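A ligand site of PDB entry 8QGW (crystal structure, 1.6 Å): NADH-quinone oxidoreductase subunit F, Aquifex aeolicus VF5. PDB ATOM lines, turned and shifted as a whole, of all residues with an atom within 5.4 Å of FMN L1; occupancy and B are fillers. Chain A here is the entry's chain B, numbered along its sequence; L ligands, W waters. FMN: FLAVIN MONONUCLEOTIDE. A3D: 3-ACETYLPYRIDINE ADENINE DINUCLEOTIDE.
Water W6 lies within hydrogen-bond range of an oxygen (O3P) of FMN L1 (2.7 Å), the backbone NH of Phe 71 (2.9 Å) and the backbone NH of Gly 70 (3.4 Å). Water W5 lies within hydrogen-bond range of O2P of FMN L1 (2.7 Å), N of Ala 69 (2.9 Å) and N of Gly 68 (3.3 Å). Water W4 lies within hydrogen-bond range of an oxygen (O3P) of FMN L1, the backbone carbonyl oxygen of Phe 71, the side-chain hydroxyl of Thr 73, the side-chain amide nitrogen of Asn 219 and the backbone NH of Gly 65. Water W3 lies within hydrogen-bond range of O4 of FMN L1 (2.8 Å), N of Glu 97 (3.0 Å) and N of Ser 96 (3.1 Å).
The side-chain hydroxyl (OG1) of Thr 223 is in hydrogen-bond range of an oxygen (O1P) of FMN L1 (2.6 Å). The side-chain amino group (NZ) of Lys 76 is in salt-bridge range of an oxygen (O3P) of FMN L1, at 2.7 Å. N of Gly 67 sits at hydrogen-bond distance from O2P of FMN L1 (2.8 Å). O1P of FMN L1 lies within hydrogen-bond range of N of Asn 220, at 2.9 Å. The side-chain amide nitrogen (ND2) of Asn 220 lies within hydrogen-bond range of an oxygen (O2) of FMN L1, at 2.8 Å. An oxygen (O1P) of FMN L1 lies within hydrogen-bond range of the side-chain amide nitrogen (ND2) of Asn 219 (2.9 Å). O2' of FMN L1 sits at hydrogen-bond distance from N of Glu 185, at 3.0 Å. The side-chain amide nitrogen of Asn 92 sits at hydrogen-bond distance from an oxygen (O4') of FMN L1, 3.1 Å away. The backbone NH (N) of Glu 95 is in hydrogen-bond range of an oxygen (O4) of FMN L1, 3.1 Å away. An oxygen (O2P) of FMN L1 sits at hydrogen-bond distance from the backbone NH (N) of Arg 66 (3.3 Å). NZ of Lys 76 lies within hydrogen-bond range of O3B of A3D L2 (2.8 Å). The side-chain carboxylate (OE2) of Glu 185 lies within hydrogen-bond range of an oxygen (O2B) of A3D L2, 2.5 Å away. O of Gly 68 sits at hydrogen-bond distance from O3D of A3D L2, 3.1 Å away.
N10 of FMN L1 sits close to O of Gly 183 (3.2 Å). The backbone carbonyl oxygen (O) of Val 218 sits close to an oxygen (O5') of FMN L1 (3.4 Å). Residues that only touch FMN L1: Gly 65 (3.4 Å), Asp 94 (3.6 Å), Ser 96 (3.9 Å), Tyr 180 (3.5 Å), Ile 181 (3.8 Å), Glu 184 (3.6 Å), Gly 394 (3.8 Å) and Leu 395 (3.9 Å). Of the 28 residues printed, 19 come within 4 Å of FMN L1. The nearest printed residue that does not touch FMN L1 is Gly 68 (4.2 Å).
An oxygen (O1N) of A3D L2 sits at hydrogen-bond distance from an oxygen (O3') of FMN L1.
OG1 of Thr 223 lies within hydrogen-bond range of N of Arg 66. The side-chain amino group of Lys 76 lies close to the side-chain amide nitrogen of Asn 219 (3.5 Å). The backbone carbonyl oxygen (O) of Asn 219 lies within hydrogen-bond range of the backbone NH (N) of Asn 92 (2.8 Å). ND2 of Asn 92 is in hydrogen-bond range of O of Gly 183 (2.8 Å). The side-chain amide oxygen (OD1) of Asn 92 lies within hydrogen-bond range of the backbone NH (N) of Asp 94 (3.1 Å). N of Gly 183 sits at hydrogen-bond distance from OD2 of Asp 94, at 3.2 Å. The backbone carbonyl oxygen (O) of Gly 65 lies close to the backbone NH (N) of Gly 70 (3.5 Å). The side-chain sulfur of Cys 393 sits close to the backbone NH of Leu 395, at 3.4 Å.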
ATOM      1  N   GLY A  65      20.659 -20.757 -13.735  1.00  0.00           N
ATOM      2  CA  GLY A  65      19.642 -21.591 -14.332  1.00  0.00           C
ATOM      3  C   GLY A  65      19.832 -21.789 -15.833  1.00  0.00           C
ATOM      4  O   GLY A  65      20.109 -20.829 -16.573  1.00  0.00           O
ATOM      5  N   ARG A  66      19.654 -23.047 -16.268  1.00  0.00           N
ATOM      6  CA  ARG A  66      19.831 -23.420 -17.656  1.00  0.00           C
ATOM      7  C   ARG A  66      18.489 -23.605 -18.383  1.00  0.00           C
ATOM      8  O   ARG A  66      18.480 -24.019 -19.547  1.00  0.00           O
ATOM      9  CB  ARG A  66      20.653 -24.713 -17.719  1.00  0.00           C
ATOM     10  CG  ARG A  66      22.024 -24.601 -17.060  1.00  0.00           C
ATOM     11  CD  ARG A  66      23.043 -23.834 -17.850  1.00  0.00           C
ATOM     12  NE  ARG A  66      24.407 -24.090 -17.405  1.00  0.00           N
ATOM     13  CZ  ARG A  66      25.219 -23.247 -16.789  1.00  0.00           C
ATOM     14  NH1 ARG A  66      26.500 -23.572 -16.632  1.00  0.00           N
ATOM     15  NH2 ARG A  66      24.767 -22.079 -16.367  1.00  0.00           N
ATOM     16  N   GLY A  67      17.367 -23.274 -17.729  1.00  0.00           N
ATOM     17  CA  GLY A  67      16.055 -23.456 -18.367  1.00  0.00           C
ATOM     18  C   GLY A  67      15.578 -22.206 -19.106  1.00  0.00           C
ATOM     19  O   GLY A  67      14.446 -22.199 -19.582  1.00  0.00           O
ATOM     20  N   GLY A  68      16.424 -21.162 -19.144  1.00  0.00           N
ATOM     21  CA  GLY A  68      16.188 -20.024 -20.015  1.00  0.00           C
ATOM     22  C   GLY A  68      16.343 -18.661 -19.341  1.00  0.00           C
ATOM     23  O   GLY A  68      16.666 -17.683 -20.037  1.00  0.00           O
ATOM     24  N   ALA A  69      16.121 -18.550 -18.015  1.00  0.00           N
ATOM     25  CA  ALA A  69      16.088 -17.244 -17.348  1.00  0.00           C
ATOM     26  C   ALA A  69      17.392 -16.906 -16.626  1.00  0.00           C
ATOM     27  O   ALA A  69      17.595 -15.756 -16.223  1.00  0.00           O
ATOM     28  CB  ALA A  69      14.932 -17.195 -16.385  1.00  0.00           C
ATOM     29  N   GLY A  70      18.262 -17.900 -16.383  1.00  0.00           N
ATOM     30  CA  GLY A  70      19.584 -17.611 -15.830  1.00  0.00           C
ATOM     31  C   GLY A  70      19.620 -17.139 -14.381  1.00  0.00           C
ATOM     32  O   GLY A  70      20.583 -16.459 -13.976  1.00  0.00           O
ATOM     33  N   PHE A  71      18.616 -17.501 -13.565  1.00  0.00           N
ATOM     34  CA  PHE A  71      18.587 -17.092 -12.171  1.00  0.00           C
ATOM     35  C   PHE A  71      19.689 -17.847 -11.428  1.00  0.00           C
ATOM     36  O   PHE A  71      19.900 -19.049 -11.647  1.00  0.00           O
ATOM     37  CB  PHE A  71      17.233 -17.344 -11.505  1.00  0.00           C
ATOM     38  CG  PHE A  71      17.068 -16.666 -10.159  1.00  0.00           C
ATOM     39  CD1 PHE A  71      16.602 -15.353 -10.059  1.00  0.00           C
ATOM     40  CD2 PHE A  71      17.404 -17.313  -8.991  1.00  0.00           C
ATOM     41  CE1 PHE A  71      16.444 -14.749  -8.816  1.00  0.00           C
ATOM     42  CE2 PHE A  71      17.254 -16.699  -7.756  1.00  0.00           C
ATOM     43  CZ  PHE A  71      16.816 -15.401  -7.673  1.00  0.00           C
ATOM     44  N   THR A  73      21.508 -20.196  -9.111  1.00  0.00           N
ATOM     45  CA  THR A  73      20.917 -21.393  -8.527  1.00  0.00           C
ATOM     46  C   THR A  73      21.085 -21.433  -7.008  1.00  0.00           C
ATOM     47  O   THR A  73      20.132 -21.773  -6.292  1.00  0.00           O
ATOM     48  CB  THR A  73      21.547 -22.637  -9.182  1.00  0.00           C
ATOM     49  OG1 THR A  73      21.412 -22.502 -10.596  1.00  0.00           O
ATOM     50  CG2 THR A  73      20.889 -23.912  -8.728  1.00  0.00           C
ATOM     51  N   LYS A  76      18.640 -19.180  -5.386  1.00  0.00           N
ATOM     52  CA  LYS A  76      17.297 -19.718  -5.404  1.00  0.00           C
ATOM     53  C   LYS A  76      17.131 -20.668  -4.205  1.00  0.00           C
ATOM     54  O   LYS A  76      16.147 -20.581  -3.468  1.00  0.00           O
ATOM     55  CB  LYS A  76      16.999 -20.437  -6.720  1.00  0.00           C
ATOM     56  CG  LYS A  76      15.532 -20.806  -6.892  1.00  0.00           C
ATOM     57  CD  LYS A  76      15.205 -21.669  -8.082  1.00  0.00           C
ATOM     58  CE  LYS A  76      15.611 -21.077  -9.423  1.00  0.00           C
ATOM     59  NZ  LYS A  76      15.065 -21.874 -10.544  1.00  0.00           N
ATOM     60  N   ASN A  92      12.700 -29.922 -13.715  1.00  0.00           N
ATOM     61  CA  ASN A  92      11.922 -29.567 -14.898  1.00  0.00           C
ATOM     62  C   ASN A  92      12.531 -30.231 -16.138  1.00  0.00           C
ATOM     63  O   ASN A  92      13.543 -29.745 -16.643  1.00  0.00           O
ATOM     64  CB  ASN A  92      11.861 -28.048 -15.031  1.00  0.00           C
ATOM     65  CG  ASN A  92      10.861 -27.568 -16.045  1.00  0.00           C
ATOM     66  OD1 ASN A  92      10.490 -28.329 -16.938  1.00  0.00           O
ATOM     67  ND2 ASN A  92      10.455 -26.301 -15.888  1.00  0.00           N
ATOM     68  N   ASP A  94      10.525 -30.659 -18.927  1.00  0.00           N
ATOM     69  CA  ASP A  94       9.431 -30.493 -19.887  1.00  0.00           C
ATOM     70  C   ASP A  94       9.907 -30.159 -21.316  1.00  0.00           C
ATOM     71  O   ASP A  94       9.127 -30.277 -22.254  1.00  0.00           O
ATOM     72  CB  ASP A  94       8.410 -29.429 -19.447  1.00  0.00           C
ATOM     73  CG  ASP A  94       7.077 -29.650 -20.157  1.00  0.00           C
ATOM     74  OD1 ASP A  94       6.492 -30.743 -20.010  1.00  0.00           O
ATOM     75  OD2 ASP A  94       6.664 -28.746 -20.928  1.00  0.00           O
ATOM     76  N   GLU A  95      11.159 -29.717 -21.436  1.00  0.00           N
ATOM     77  CA  GLU A  95      11.832 -29.340 -22.671  1.00  0.00           C
ATOM     78  C   GLU A  95      10.964 -29.451 -23.927  1.00  0.00           C
ATOM     79  O   GLU A  95      10.943 -30.486 -24.583  1.00  0.00           O
ATOM     80  CB  GLU A  95      13.116 -30.166 -22.800  1.00  0.00           C
ATOM     81  CG  GLU A  95      13.868 -29.857 -24.071  1.00  0.00           C
ATOM     82  CD  GLU A  95      15.244 -30.469 -24.085  1.00  0.00           C
ATOM     83  OE1 GLU A  95      15.304 -31.700 -24.237  1.00  0.00           O
ATOM     84  OE2 GLU A  95      16.243 -29.683 -23.903  1.00  0.00           O
ATOM     85  N   SER A  96      10.287 -28.341 -24.287  1.00  0.00           N
ATOM     86  CA  SER A  96       9.366 -28.370 -25.407  1.00  0.00           C
ATOM     87  C   SER A  96       9.500 -27.129 -26.298  1.00  0.00           C
ATOM     88  O   SER A  96       8.696 -27.000 -27.213  1.00  0.00           O
ATOM     89  CB  SER A  96       7.913 -28.505 -24.898  1.00  0.00           C
ATOM     90  OG  SER A  96       7.676 -29.829 -24.445  1.00  0.00           O
ATOM     91  N   GLU A  97      10.461 -26.230 -26.034  1.00  0.00           N
ATOM     92  CA  GLU A  97      10.634 -25.071 -26.909  1.00  0.00           C
ATOM     93  C   GLU A  97      11.250 -25.513 -28.235  1.00  0.00           C
ATOM     94  O   GLU A  97      12.217 -26.283 -28.247  1.00  0.00           O
ATOM     95  CB  GLU A  97      11.557 -24.035 -26.269  1.00  0.00           C
ATOM     96  CG  GLU A  97      11.575 -22.735 -27.051  1.00  0.00           C
ATOM     97  CD  GLU A  97      12.320 -21.573 -26.429  1.00  0.00           C
ATOM     98  OE1 GLU A  97      12.715 -21.648 -25.219  1.00  0.00           O
ATOM     99  OE2 GLU A  97      12.491 -20.585 -27.145  1.00  0.00           O
ATOM    100  N   ASP A 103      18.306 -31.315 -23.014  1.00  0.00           N
ATOM    101  CA  ASP A 103      18.039 -31.982 -21.739  1.00  0.00           C
ATOM    102  C   ASP A 103      17.838 -33.483 -21.938  1.00  0.00           C
ATOM    103  O   ASP A 103      18.267 -34.289 -21.117  1.00  0.00           O
ATOM    104  CB  ASP A 103      16.808 -31.386 -21.055  1.00  0.00           C
ATOM    105  CG  ASP A 103      16.998 -29.949 -20.579  1.00  0.00           C
ATOM    106  OD1 ASP A 103      18.150 -29.487 -20.541  1.00  0.00           O
ATOM    107  OD2 ASP A 103      15.967 -29.298 -20.279  1.00  0.00           O
ATOM    108  N   TYR A 180       3.150 -27.174 -23.820  1.00  0.00           N
ATOM    109  CA  TYR A 180       4.409 -26.455 -23.636  1.00  0.00           C
ATOM    110  C   TYR A 180       4.382 -25.596 -22.376  1.00  0.00           C
ATOM    111  O   TYR A 180       5.403 -25.437 -21.701  1.00  0.00           O
ATOM    112  CB  TYR A 180       4.670 -25.530 -24.840  1.00  0.00           C
ATOM    113  CG  TYR A 180       5.757 -24.513 -24.634  1.00  0.00           C
ATOM    114  CD1 TYR A 180       7.076 -24.861 -24.524  1.00  0.00           C
ATOM    115  CD2 TYR A 180       5.453 -23.155 -24.595  1.00  0.00           C
ATOM    116  CE1 TYR A 180       8.082 -23.928 -24.349  1.00  0.00           C
ATOM    117  CE2 TYR A 180       6.445 -22.209 -24.431  1.00  0.00           C
ATOM    118  CZ  TYR A 180       7.770 -22.580 -24.303  1.00  0.00           C
ATOM    119  OH  TYR A 180       8.741 -21.622 -24.090  1.00  0.00           O
ATOM    120  N   ILE A 181       3.192 -25.122 -21.994  1.00  0.00           N
ATOM    121  CA  ILE A 181       3.075 -24.199 -20.868  1.00  0.00           C
ATOM    122  C   ILE A 181       3.415 -24.926 -19.567  1.00  0.00           C
ATOM    123  O   ILE A 181       3.757 -24.296 -18.588  1.00  0.00           O
ATOM    124  CB  ILE A 181       1.697 -23.513 -20.802  1.00  0.00           C
ATOM    125  CG1 ILE A 181       1.685 -22.327 -19.829  1.00  0.00           C
ATOM    126  CG2 ILE A 181       0.583 -24.492 -20.459  1.00  0.00           C
ATOM    127  CD1 ILE A 181       2.722 -21.279 -20.146  1.00  0.00           C
ATOM    128  N   GLY A 183       6.029 -26.373 -18.925  1.00  0.00           N
ATOM    129  CA  GLY A 183       7.411 -26.048 -18.581  1.00  0.00           C
ATOM    130  C   GLY A 183       7.558 -24.778 -17.747  1.00  0.00           C
ATOM    131  O   GLY A 183       8.565 -24.575 -17.109  1.00  0.00           O
ATOM    132  N   GLU A 184       6.547 -23.914 -17.740  1.00  0.00           N
ATOM    133  CA  GLU A 184       6.567 -22.763 -16.849  1.00  0.00           C
ATOM    134  C   GLU A 184       6.396 -23.311 -15.441  1.00  0.00           C
ATOM    135  O   GLU A 184       5.487 -24.105 -15.222  1.00  0.00           O
ATOM    136  CB  GLU A 184       5.458 -21.801 -17.271  1.00  0.00           C
ATOM    137  CG  GLU A 184       5.609 -20.405 -16.696  1.00  0.00           C
ATOM    138  CD  GLU A 184       5.133 -20.188 -15.272  1.00  0.00           C
ATOM    139  OE1 GLU A 184       4.430 -21.043 -14.699  1.00  0.00           O
ATOM    140  OE2 GLU A 184       5.479 -19.092 -14.724  1.00  0.00           O
ATOM    141  N   GLU A 185       7.252 -22.917 -14.515  1.00  0.00           N
ATOM    142  CA  GLU A 185       7.412 -23.644 -13.263  1.00  0.00           C
ATOM    143  C   GLU A 185       6.094 -23.707 -12.475  1.00  0.00           C
ATOM    144  O   GLU A 185       5.864 -24.692 -11.760  1.00  0.00           O
ATOM    145  CB  GLU A 185       8.520 -23.027 -12.402  1.00  0.00           C
ATOM    146  CG  GLU A 185       8.315 -21.553 -12.148  1.00  0.00           C
ATOM    147  CD  GLU A 185       9.352 -20.894 -11.265  1.00  0.00           C
ATOM    148  OE1 GLU A 185      10.347 -21.590 -10.887  1.00  0.00           O
ATOM    149  OE2 GLU A 185       9.172 -19.709 -10.980  1.00  0.00           O
ATOM    150  N   VAL A 218      12.262 -25.295  -8.228  1.00  0.00           N
ATOM    151  CA  VAL A 218      12.239 -25.857  -9.574  1.00  0.00           C
ATOM    152  C   VAL A 218      13.557 -25.518 -10.245  1.00  0.00           C
ATOM    153  O   VAL A 218      13.950 -24.335 -10.294  1.00  0.00           O
ATOM    154  CB  VAL A 218      11.045 -25.343 -10.386  1.00  0.00           C
ATOM    155  CG1 VAL A 218      11.013 -25.991 -11.758  1.00  0.00           C
ATOM    156  CG2 VAL A 218       9.726 -25.553  -9.643  1.00  0.00           C
ATOM    157  N   ASN A 219      14.235 -26.557 -10.774  1.00  0.00           N
ATOM    158  CA  ASN A 219      15.442 -26.371 -11.555  1.00  0.00           C
ATOM    159  C   ASN A 219      15.373 -27.243 -12.805  1.00  0.00           C
ATOM    160  O   ASN A 219      14.797 -28.325 -12.799  1.00  0.00           O
ATOM    161  CB  ASN A 219      16.723 -26.682 -10.785  1.00  0.00           C
ATOM    162  CG  ASN A 219      17.247 -25.553  -9.925  1.00  0.00           C
ATOM    163  OD1 ASN A 219      17.428 -25.721  -8.714  1.00  0.00           O
ATOM    164  ND2 ASN A 219      17.441 -24.379 -10.524  1.00  0.00           N
ATOM    165  N   ASN A 220      16.000 -26.731 -13.842  1.00  0.00           N
ATOM    166  CA  ASN A 220      16.098 -27.392 -15.137  1.00  0.00           C
ATOM    167  C   ASN A 220      17.062 -28.586 -15.062  1.00  0.00           C
ATOM    168  O   ASN A 220      18.035 -28.555 -14.313  1.00  0.00           O
ATOM    169  CB  ASN A 220      16.592 -26.356 -16.161  1.00  0.00           C
ATOM    170  CG  ASN A 220      16.934 -26.958 -17.498  1.00  0.00           C
ATOM    171  OD1 ASN A 220      18.104 -27.139 -17.807  1.00  0.00           O
ATOM    172  ND2 ASN A 220      15.909 -27.324 -18.260  1.00  0.00           N
ATOM    173  N   VAL A 221      16.819 -29.581 -15.924  1.00  0.00           N
ATOM    174  CA  VAL A 221      17.652 -30.778 -16.042  1.00  0.00           C
ATOM    175  C   VAL A 221      19.142 -30.407 -16.092  1.00  0.00           C
ATOM    176  O   VAL A 221      19.971 -30.959 -15.363  1.00  0.00           O
ATOM    177  CB  VAL A 221      17.247 -31.600 -17.273  1.00  0.00           C
ATOM    178  CG1 VAL A 221      18.283 -32.666 -17.617  1.00  0.00           C
ATOM    179  CG2 VAL A 221      15.878 -32.236 -17.115  1.00  0.00           C
ATOM    180  N   THR A 223      20.733 -27.578 -15.377  1.00  0.00           N
ATOM    181  CA  THR A 223      21.211 -26.966 -14.154  1.00  0.00           C
ATOM    182  C   THR A 223      21.644 -28.033 -13.136  1.00  0.00           C
ATOM    183  O   THR A 223      22.728 -27.989 -12.558  1.00  0.00           O
ATOM    184  CB  THR A 223      20.144 -26.074 -13.492  1.00  0.00           C
ATOM    185  OG1 THR A 223      19.477 -25.299 -14.503  1.00  0.00           O
ATOM    186  CG2 THR A 223      20.735 -25.185 -12.408  1.00  0.00           C
ATOM    187  N   CYS A 393       2.396 -14.739 -17.216  1.00  0.00           N
ATOM    188  CA  CYS A 393       3.597 -15.560 -17.342  1.00  0.00           C
ATOM    189  C   CYS A 393       4.397 -15.124 -18.562  1.00  0.00           C
ATOM    190  O   CYS A 393       3.994 -14.259 -19.347  1.00  0.00           O
ATOM    191  CB  CYS A 393       3.301 -17.068 -17.386  1.00  0.00           C
ATOM    192  SG  CYS A 393       3.005 -17.777 -19.031  1.00  0.00           S
ATOM    193  N   GLY A 394       5.589 -15.715 -18.683  1.00  0.00           N
ATOM    194  CA  GLY A 394       6.546 -15.308 -19.709  1.00  0.00           C
ATOM    195  C   GLY A 394       6.083 -15.531 -21.136  1.00  0.00           C
ATOM    196  O   GLY A 394       6.639 -14.911 -22.046  1.00  0.00           O
ATOM    197  N   LEU A 395       5.132 -16.462 -21.361  1.00  0.00           N
ATOM    198  CA  LEU A 395       4.746 -16.794 -22.727  1.00  0.00           C
ATOM    199  C   LEU A 395       4.137 -15.542 -23.380  1.00  0.00           C
ATOM    200  O   LEU A 395       4.563 -15.128 -24.465  1.00  0.00           O
ATOM    201  CB  LEU A 395       3.793 -17.994 -22.757  1.00  0.00           C
ATOM    202  CG  LEU A 395       3.456 -18.537 -24.157  1.00  0.00           C
ATOM    203  CD1 LEU A 395       3.108 -20.017 -24.094  1.00  0.00           C
ATOM    204  CD2 LEU A 395       2.260 -17.790 -24.746  1.00  0.00           C
HETATM  205  N1  FMN L   1      12.222 -24.325 -17.775  1.00  0.00           N
HETATM  206  C2  FMN L   1      12.685 -25.573 -18.000  1.00  0.00           C
HETATM  207  O2  FMN L   1      13.546 -26.108 -17.231  1.00  0.00           O
HETATM  208  N3  FMN L   1      12.140 -26.338 -19.023  1.00  0.00           N
HETATM  209  C4  FMN L   1      11.100 -25.942 -19.873  1.00  0.00           C
HETATM  210  O4  FMN L   1      10.671 -26.713 -20.728  1.00  0.00           O
HETATM  211  C4A FMN L   1      10.599 -24.605 -19.611  1.00  0.00           C
HETATM  212  N5  FMN L   1       9.578 -24.165 -20.325  1.00  0.00           N
HETATM  213  C5A FMN L   1       9.090 -22.893 -20.040  1.00  0.00           C
HETATM  214  C6  FMN L   1       7.985 -22.413 -20.735  1.00  0.00           C
HETATM  215  C7  FMN L   1       7.461 -21.144 -20.488  1.00  0.00           C
HETATM  216  C7M FMN L   1       6.265 -20.664 -21.264  1.00  0.00           C
HETATM  217  C8  FMN L   1       8.064 -20.339 -19.518  1.00  0.00           C
HETATM  218  C8M FMN L   1       7.638 -18.907 -19.328  1.00  0.00           C
HETATM  219  C9  FMN L   1       9.163 -20.809 -18.802  1.00  0.00           C
HETATM  220  C9A FMN L   1       9.678 -22.072 -19.050  1.00  0.00           C
HETATM  221  N10 FMN L   1      10.766 -22.589 -18.323  1.00  0.00           N
HETATM  222  C10 FMN L   1      11.237 -23.862 -18.561  1.00  0.00           C
HETATM  223  C1' FMN L   1      11.404 -21.809 -17.267  1.00  0.00           C
HETATM  224  C2' FMN L   1      10.853 -22.203 -15.884  1.00  0.00           C
HETATM  225  O2' FMN L   1       9.655 -21.459 -15.595  1.00  0.00           O
HETATM  226  C3' FMN L   1      11.913 -21.969 -14.806  1.00  0.00           C
HETATM  227  O3' FMN L   1      12.555 -20.699 -14.881  1.00  0.00           O
HETATM  228  C4' FMN L   1      13.037 -23.009 -14.734  1.00  0.00           C
HETATM  229  O4' FMN L   1      12.559 -24.346 -14.810  1.00  0.00           O
HETATM  230  C5' FMN L   1      13.862 -22.820 -13.474  1.00  0.00           C
HETATM  231  O5' FMN L   1      15.012 -23.680 -13.482  1.00  0.00           O
HETATM  232  P   FMN L   1      16.476 -23.043 -13.733  1.00  0.00           P
HETATM  233  O1P FMN L   1      17.401 -24.228 -13.436  1.00  0.00           O
HETATM  234  O2P FMN L   1      16.549 -22.604 -15.178  1.00  0.00           O
HETATM  235  O3P FMN L   1      16.661 -21.908 -12.747  1.00  0.00           O
HETATM  236  PA  A3D L   2      11.853 -15.718 -14.194  1.00  0.00           P
HETATM  237  O1A A3D L   2      12.947 -14.782 -14.516  1.00  0.00           O
HETATM  238  O2A A3D L   2      10.548 -15.200 -13.704  1.00  0.00           O
HETATM  239  O5B A3D L   2      12.378 -16.710 -13.061  1.00  0.00           O
HETATM  240  C5B A3D L   2      13.519 -17.559 -13.286  1.00  0.00           C
HETATM  241  C4B A3D L   2      13.703 -18.450 -12.086  1.00  0.00           C
HETATM  242  O4B A3D L   2      14.180 -17.696 -10.955  1.00  0.00           O
HETATM  243  C3B A3D L   2      12.423 -19.122 -11.595  1.00  0.00           C
HETATM  244  O3B A3D L   2      12.707 -20.410 -11.037  1.00  0.00           O
HETATM  245  C2B A3D L   2      11.895 -18.146 -10.537  1.00  0.00           C
HETATM  246  O2B A3D L   2      11.022 -18.735  -9.554  1.00  0.00           O
HETATM  247  C1B A3D L   2      13.208 -17.672  -9.915  1.00  0.00           C
HETATM  248  N9A A3D L   2      13.142 -16.312  -9.392  1.00  0.00           N
HETATM  249  C8A A3D L   2      13.081 -15.150 -10.119  1.00  0.00           C
HETATM  250  N7A A3D L   2      12.932 -14.068  -9.399  1.00  0.00           N
HETATM  251  C5A A3D L   2      12.893 -14.549  -8.097  1.00  0.00           C
HETATM  252  C6A A3D L   2      12.798 -13.906  -6.836  1.00  0.00           C
HETATM  253  N6A A3D L   2      12.705 -12.580  -6.675  1.00  0.00           N
HETATM  254  N1A A3D L   2      12.852 -14.680  -5.727  1.00  0.00           N
HETATM  255  C2A A3D L   2      12.979 -16.007  -5.881  1.00  0.00           C
HETATM  256  N3A A3D L   2      13.074 -16.719  -6.998  1.00  0.00           N
HETATM  257  C4A A3D L   2      13.024 -15.933  -8.073  1.00  0.00           C
HETATM  258  O3  A3D L   2      11.657 -16.634 -15.467  1.00  0.00           O
HETATM  259  PN  A3D L   2      10.550 -17.652 -15.998  1.00  0.00           P
HETATM  260  O1N A3D L   2      10.528 -18.821 -15.103  1.00  0.00           O
HETATM  261  O2N A3D L   2       9.320 -16.883 -16.332  1.00  0.00           O
HETATM  262  O5D A3D L   2      11.216 -18.150 -17.375  1.00  0.00           O
HETATM  263  C5D A3D L   2      11.417 -17.266 -18.515  1.00  0.00           C
HETATM  264  C4D A3D L   2      12.323 -17.898 -19.542  1.00  0.00           C
HETATM  265  O4D A3D L   2      11.678 -19.070 -20.113  1.00  0.00           O
HETATM  266  C3D A3D L   2      12.668 -16.989 -20.720  1.00  0.00           C
HETATM  267  O3D A3D L   2      13.900 -16.349 -20.461  1.00  0.00           O
HETATM  268  C2D A3D L   2      12.794 -17.956 -21.893  1.00  0.00           C
HETATM  269  O2D A3D L   2      14.080 -18.536 -22.013  1.00  0.00           O
HETATM  270  C1D A3D L   2      11.804 -19.067 -21.514  1.00  0.00           C
HETATM  271  N1N A3D L   2      10.448 -18.876 -22.132  1.00  0.00           N
HETATM  272  C6N A3D L   2       9.940 -17.646 -22.323  1.00  0.00           C
HETATM  273  O   HOH W   1      13.358 -29.065 -19.366  1.00  0.00           O
HETATM  274  O   HOH W   2       8.001 -26.721 -21.843  1.00  0.00           O
HETATM  275  O   HOH W   3      11.328 -25.651 -23.234  1.00  0.00           O
HETATM  276  O   HOH W   4      18.719 -21.548 -11.003  1.00  0.00           O
HETATM  277  O   HOH W   5      15.098 -20.544 -16.181  1.00  0.00           O
HETATM  278  O   HOH W   6      16.533 -19.478 -13.876  1.00  0.00           O
HETATM  279  O   HOH W   7      12.973 -23.412 -21.318  1.00  0.00           O
